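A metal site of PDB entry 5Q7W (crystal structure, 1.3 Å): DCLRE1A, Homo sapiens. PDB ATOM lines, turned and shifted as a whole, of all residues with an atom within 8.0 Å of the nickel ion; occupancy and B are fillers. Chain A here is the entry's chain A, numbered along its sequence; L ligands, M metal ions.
The backbone carbonyl oxygen (O) of Glu 296 lies within hydrogen-bond range of a ring nitrogen (ND1) of His 96, 2.8 Å away.
A ring nitrogen (ND1) of His 35 sits at hydrogen-bond distance from the side-chain hydroxyl (OG1) of Thr 34, 2.9 Å away.
O of Ile 184 is in hydrogen-bond range of NE2 of His 37.
NE2 of His 40 sits close to OD2 of Asp 118, at 3.4 Å.
NE2 of His 37 lies within hydrogen-bond range of SG of Cys 97.
Within 4 Å of the nickel ion: His 35, His 37, His 96 and Asp 118.
The nearest printed residue that does not touch the nickel ion is His 40 (4.2 Å).
The nickel ion is bound by O3 of the ligand, O2 of the ligand, OD2 of Asp 118, NE2 of His 35, ND1 of His 37 and NE2 of His 96.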
ATOM      1  N   ASP A  18       1.394  27.967  -3.784  1.00  0.00           N
ATOM      2  CA  ASP A  18       1.344  27.237  -5.068  1.00  0.00           C
ATOM      3  C   ASP A  18       2.441  27.762  -6.095  1.00  0.00           C
ATOM      4  O   ASP A  18       2.187  27.939  -7.315  1.00  0.00           O
ATOM      5  CB  ASP A  18      -0.061  27.206  -5.657  1.00  0.00           C
ATOM      6  CG  ASP A  18      -1.090  26.528  -4.718  1.00  0.00           C
ATOM      7  OD1 ASP A  18      -0.649  25.878  -3.739  1.00  0.00           O
ATOM      8  OD2 ASP A  18      -2.284  26.665  -5.079  1.00  0.00           O
ATOM      9  N   THR A  34      -1.868  24.367  -1.632  1.00  0.00           N
ATOM     10  CA  THR A  34      -3.288  24.278  -1.348  1.00  0.00           C
ATOM     11  C   THR A  34      -3.875  22.878  -1.612  1.00  0.00           C
ATOM     12  O   THR A  34      -4.796  22.459  -0.900  1.00  0.00           O
ATOM     13  CB  THR A  34      -4.127  25.328  -2.101  1.00  0.00           C
ATOM     14  OG1 THR A  34      -4.018  25.130  -3.557  1.00  0.00           O
ATOM     15  CG2 THR A  34      -3.712  26.795  -1.751  1.00  0.00           C
ATOM     16  N   HIS A  35      -3.344  22.194  -2.671  1.00  0.00           N
ATOM     17  CA  HIS A  35      -3.880  20.889  -3.106  1.00  0.00           C
ATOM     18  C   HIS A  35      -2.965  20.222  -4.048  1.00  0.00           C
ATOM     19  O   HIS A  35      -2.185  20.901  -4.756  1.00  0.00           O
ATOM     20  CB  HIS A  35      -5.360  21.037  -3.621  1.00  0.00           C
ATOM     21  CG  HIS A  35      -5.531  21.725  -4.921  1.00  0.00           C
ATOM     22  ND1 HIS A  35      -5.335  23.083  -5.118  1.00  0.00           N
ATOM     23  CD2 HIS A  35      -5.957  21.235  -6.113  1.00  0.00           C
ATOM     24  CE1 HIS A  35      -5.677  23.366  -6.384  1.00  0.00           C
ATOM     25  NE2 HIS A  35      -6.066  22.261  -6.979  1.00  0.00           N
ATOM     26  N   PHE A  36      -3.166  18.908  -4.145  1.00  0.00           N
ATOM     27  CA  PHE A  36      -2.321  18.083  -5.089  1.00  0.00           C
ATOM     28  C   PHE A  36      -2.864  17.975  -6.526  1.00  0.00           C
ATOM     29  O   PHE A  36      -3.305  16.840  -6.964  1.00  0.00           O
ATOM     30  CB  PHE A  36      -2.130  16.649  -4.442  1.00  0.00           C
ATOM     31  CG  PHE A  36      -1.012  15.796  -5.045  1.00  0.00           C
ATOM     32  CD1 PHE A  36       0.271  16.125  -4.718  1.00  0.00           C
ATOM     33  CD2 PHE A  36      -1.258  14.732  -5.916  1.00  0.00           C
ATOM     34  CE1 PHE A  36       1.359  15.370  -5.203  1.00  0.00           C
ATOM     35  CE2 PHE A  36      -0.180  13.966  -6.435  1.00  0.00           C
ATOM     36  CZ  PHE A  36       1.096  14.284  -6.089  1.00  0.00           C
ATOM     37  N   HIS A  37      -2.873  19.101  -7.242  1.00  0.00           N
ATOM     38  CA  HIS A  37      -3.116  19.127  -8.690  1.00  0.00           C
ATOM     39  C   HIS A  37      -1.861  19.702  -9.385  1.00  0.00           C
ATOM     40  O   HIS A  37      -1.194  20.644  -8.878  1.00  0.00           O
ATOM     41  CB  HIS A  37      -4.362  19.964  -9.098  1.00  0.00           C
ATOM     42  CG  HIS A  37      -5.701  19.274  -8.916  1.00  0.00           C
ATOM     43  ND1 HIS A  37      -6.928  19.919  -8.896  1.00  0.00           N
ATOM     44  CD2 HIS A  37      -5.976  17.958  -8.832  1.00  0.00           C
ATOM     45  CE1 HIS A  37      -7.901  19.029  -8.808  1.00  0.00           C
ATOM     46  NE2 HIS A  37      -7.334  17.830  -8.733  1.00  0.00           N
ATOM     47  N   SER A  38      -1.522  19.117 -10.553  1.00  0.00           N
ATOM     48  CA  SER A  38      -0.185  19.338 -11.122  1.00  0.00           C
ATOM     49  C   SER A  38       0.050  20.813 -11.458  1.00  0.00           C
ATOM     50  O   SER A  38       1.248  21.229 -11.289  1.00  0.00           O
ATOM     51  CB  SER A  38       0.103  18.376 -12.301  1.00  0.00           C
ATOM     52  OG  SER A  38      -0.814  18.611 -13.342  1.00  0.00           O
ATOM     53  N   ASP A  39      -0.930  21.604 -11.907  1.00  0.00           N
ATOM     54  CA  ASP A  39      -0.628  23.050 -12.212  1.00  0.00           C
ATOM     55  C   ASP A  39      -0.182  23.793 -10.928  1.00  0.00           C
ATOM     56  O   ASP A  39       0.453  24.890 -11.014  1.00  0.00           O
ATOM     57  CB  ASP A  39      -1.820  23.769 -12.788  1.00  0.00           C
ATOM     58  CG  ASP A  39      -2.078  23.510 -14.330  1.00  0.00           C
ATOM     59  OD1 ASP A  39      -1.248  22.820 -14.939  1.00  0.00           O
ATOM     60  OD2 ASP A  39      -3.140  24.010 -14.785  1.00  0.00           O
ATOM     61  N   HIS A  40      -0.562  23.266  -9.735  1.00  0.00           N
ATOM     62  CA  HIS A  40      -0.247  23.900  -8.451  1.00  0.00           C
ATOM     63  C   HIS A  40       0.994  23.369  -7.784  1.00  0.00           C
ATOM     64  O   HIS A  40       1.793  24.174  -7.206  1.00  0.00           O
ATOM     65  CB  HIS A  40      -1.525  23.764  -7.527  1.00  0.00           C
ATOM     66  CG  HIS A  40      -2.690  24.465  -8.086  1.00  0.00           C
ATOM     67  ND1 HIS A  40      -3.150  25.680  -7.634  1.00  0.00           N
ATOM     68  CD2 HIS A  40      -3.541  24.110  -9.076  1.00  0.00           C
ATOM     69  CE1 HIS A  40      -4.173  26.068  -8.366  1.00  0.00           C
ATOM     70  NE2 HIS A  40      -4.425  25.110  -9.261  1.00  0.00           N
ATOM     71  N   HIS A  96     -13.081  21.090  -2.852  1.00  0.00           N
ATOM     72  CA  HIS A  96     -12.459  20.881  -4.202  1.00  0.00           C
ATOM     73  C   HIS A  96     -12.185  19.395  -4.285  1.00  0.00           C
ATOM     74  O   HIS A  96     -13.183  18.615  -4.271  1.00  0.00           O
ATOM     75  CB  HIS A  96     -11.260  21.814  -4.407  1.00  0.00           C
ATOM     76  CG  HIS A  96     -10.587  21.786  -5.766  1.00  0.00           C
ATOM     77  ND1 HIS A  96     -11.292  21.931  -6.942  1.00  0.00           N
ATOM     78  CD2 HIS A  96      -9.296  21.600  -6.100  1.00  0.00           C
ATOM     79  CE1 HIS A  96     -10.428  21.846  -7.962  1.00  0.00           C
ATOM     80  NE2 HIS A  96      -9.216  21.681  -7.494  1.00  0.00           N
ATOM     81  N   CYS A  97     -10.963  18.935  -4.390  1.00  0.00           N
ATOM     82  CA  CYS A  97     -10.570  17.497  -4.356  1.00  0.00           C
ATOM     83  C   CYS A  97     -10.128  17.111  -2.936  1.00  0.00           C
ATOM     84  O   CYS A  97      -9.931  17.976  -2.095  1.00  0.00           O
ATOM     85  CB  CYS A  97      -9.437  17.314  -5.398  1.00  0.00           C
ATOM     86  SG  CYS A  97      -7.861  18.209  -4.992  1.00  0.00           S
ATOM     87  N   ALA A 100      -7.754  19.357  -0.373  1.00  0.00           N
ATOM     88  CA  ALA A 100      -7.716  20.766  -0.786  1.00  0.00           C
ATOM     89  C   ALA A 100      -8.174  21.709   0.317  1.00  0.00           C
ATOM     90  O   ALA A 100      -9.206  21.479   0.943  1.00  0.00           O
ATOM     91  CB  ALA A 100      -8.490  20.971  -2.064  1.00  0.00           C
ATOM     92  N   GLY A 117      -7.329  28.998  -2.705  1.00  0.00           N
ATOM     93  CA  GLY A 117      -6.822  27.904  -3.537  1.00  0.00           C
ATOM     94  C   GLY A 117      -7.809  27.705  -4.661  1.00  0.00           C
ATOM     95  O   GLY A 117      -8.412  28.646  -5.176  1.00  0.00           O
ATOM     96  N   ASP A 118      -7.964  26.456  -5.075  1.00  0.00           N
ATOM     97  CA  ASP A 118      -9.140  26.059  -5.920  1.00  0.00           C
ATOM     98  C   ASP A 118     -10.324  25.664  -4.996  1.00  0.00           C
ATOM     99  O   ASP A 118     -10.074  24.941  -4.028  1.00  0.00           O
ATOM    100  CB  ASP A 118      -8.812  24.910  -6.877  1.00  0.00           C
ATOM    101  CG  ASP A 118      -8.002  25.257  -8.102  1.00  0.00           C
ATOM    102  OD1 ASP A 118      -7.852  26.454  -8.432  1.00  0.00           O
ATOM    103  OD2 ASP A 118      -7.654  24.297  -8.828  1.00  0.00           O
ATOM    104  N   PHE A 119     -11.516  26.147  -5.262  1.00  0.00           N
ATOM    105  CA  PHE A 119     -12.663  25.838  -4.397  1.00  0.00           C
ATOM    106  C   PHE A 119     -13.970  25.768  -5.146  1.00  0.00           C
ATOM    107  O   PHE A 119     -14.124  26.328  -6.207  1.00  0.00           O
ATOM    108  CB  PHE A 119     -12.792  26.814  -3.140  1.00  0.00           C
ATOM    109  CG  PHE A 119     -13.510  28.178  -3.320  1.00  0.00           C
ATOM    110  CD1 PHE A 119     -14.300  28.714  -2.321  1.00  0.00           C
ATOM    111  CD2 PHE A 119     -13.345  28.968  -4.475  1.00  0.00           C
ATOM    112  CE1 PHE A 119     -14.870  29.964  -2.415  1.00  0.00           C
ATOM    113  CE2 PHE A 119     -13.960  30.206  -4.577  1.00  0.00           C
ATOM    114  CZ  PHE A 119     -14.736  30.676  -3.543  1.00  0.00           C
ATOM    115  N   ASP A 141     -10.342  31.993  -6.546  1.00  0.00           N
ATOM    116  CA  ASP A 141     -10.404  31.050  -7.737  1.00  0.00           C
ATOM    117  C   ASP A 141     -11.591  31.531  -8.571  1.00  0.00           C
ATOM    118  O   ASP A 141     -12.776  31.282  -8.306  1.00  0.00           O
ATOM    119  CB  ASP A 141     -10.668  29.611  -7.254  1.00  0.00           C
ATOM    120  CG  ASP A 141     -11.107  28.636  -8.348  1.00  0.00           C
ATOM    121  OD1 ASP A 141     -10.940  28.991  -9.535  1.00  0.00           O
ATOM    122  OD2 ASP A 141     -11.573  27.523  -7.945  1.00  0.00           O
ATOM    123  N   THR A 143     -12.113  30.568 -11.844  1.00  0.00           N
ATOM    124  CA  THR A 143     -12.212  29.703 -12.999  1.00  0.00           C
ATOM    125  C   THR A 143     -13.467  29.938 -13.821  1.00  0.00           C
ATOM    126  O   THR A 143     -13.362  30.132 -15.105  1.00  0.00           O
ATOM    127  CB  THR A 143     -12.121  28.186 -12.535  1.00  0.00           C
ATOM    128  OG1 THR A 143     -10.853  27.881 -11.937  1.00  0.00           O
ATOM    129  CG2 THR A 143     -12.280  27.227 -13.736  1.00  0.00           C
ATOM    130  N   SER A 183      -6.397  12.810 -12.516  1.00  0.00           N
ATOM    131  CA  SER A 183      -5.947  13.534 -11.343  1.00  0.00           C
ATOM    132  C   SER A 183      -6.808  13.049 -10.178  1.00  0.00           C
ATOM    133  O   SER A 183      -7.866  12.378 -10.387  1.00  0.00           O
ATOM    134  CB  SER A 183      -6.149  15.055 -11.500  1.00  0.00           C
ATOM    135  OG  SER A 183      -7.512  15.387 -11.703  1.00  0.00           O
ATOM    136  N   ILE A 184      -6.483  13.403  -8.969  1.00  0.00           N
ATOM    137  CA  ILE A 184      -7.393  13.209  -7.866  1.00  0.00           C
ATOM    138  C   ILE A 184      -8.571  14.192  -7.979  1.00  0.00           C
ATOM    139  O   ILE A 184      -8.512  15.216  -8.750  1.00  0.00           O
ATOM    140  CB  ILE A 184      -6.720  13.395  -6.473  1.00  0.00           C
ATOM    141  CG1 ILE A 184      -6.246  14.813  -6.175  1.00  0.00           C
ATOM    142  CG2 ILE A 184      -5.617  12.370  -6.271  1.00  0.00           C
ATOM    143  CD1 ILE A 184      -5.881  15.037  -4.735  1.00  0.00           C
ATOM    144  N   GLU A 296     -15.827  20.551  -9.596  1.00  0.00           N
ATOM    145  CA  GLU A 296     -15.206  20.854  -8.284  1.00  0.00           C
ATOM    146  C   GLU A 296     -14.739  22.340  -8.153  1.00  0.00           C
ATOM    147  O   GLU A 296     -13.921  22.701  -7.285  1.00  0.00           O
ATOM    148  CB  GLU A 296     -14.125  19.856  -7.883  1.00  0.00           C
ATOM    149  CG  GLU A 296     -14.718  18.431  -7.609  1.00  0.00           C
ATOM    150  CD  GLU A 296     -13.760  17.373  -7.082  1.00  0.00           C
ATOM    151  OE1 GLU A 296     -12.523  17.502  -7.280  1.00  0.00           O
ATOM    152  OE2 GLU A 296     -14.250  16.342  -6.485  1.00  0.00           O
ATOM    153  N   HIS A 297     -15.284  23.174  -9.078  1.00  0.00           N
ATOM    154  CA  HIS A 297     -15.142  24.647  -8.947  1.00  0.00           C
ATOM    155  C   HIS A 297     -16.518  25.325  -8.842  1.00  0.00           C
ATOM    156  O   HIS A 297     -17.549  24.836  -9.350  1.00  0.00           O
ATOM    157  CB  HIS A 297     -14.386  25.252 -10.218  1.00  0.00           C
ATOM    158  CG  HIS A 297     -12.967  24.823 -10.376  1.00  0.00           C
ATOM    159  ND1 HIS A 297     -11.905  25.464  -9.796  1.00  0.00           N
ATOM    160  CD2 HIS A 297     -12.439  23.842 -11.200  1.00  0.00           C
ATOM    161  CE1 HIS A 297     -10.783  24.871 -10.169  1.00  0.00           C
ATOM    162  NE2 HIS A 297     -11.102  23.882 -10.993  1.00  0.00           N
HETATM  163  C1  LIG L   1      -7.144  21.531 -12.065  1.00  0.00           C
HETATM  164  C2  LIG L   1      -8.556  21.944 -11.656  1.00  0.00           C
HETATM  165  C3  LIG L   1      -6.045  22.402 -11.446  1.00  0.00           C
HETATM  166  O1  LIG L   1      -9.480  22.211 -12.448  1.00  0.00           O
HETATM  167  O2  LIG L   1      -8.762  21.990 -10.456  1.00  0.00           O
HETATM  168  O3  LIG L   1      -5.975  22.569 -10.202  1.00  0.00           O
HETATM  169  O4  LIG L   1      -5.112  22.859 -12.167  1.00  0.00           O
HETATM  170 NI    NI M   1      -7.378  22.113  -8.787  1.00  0.00          NI
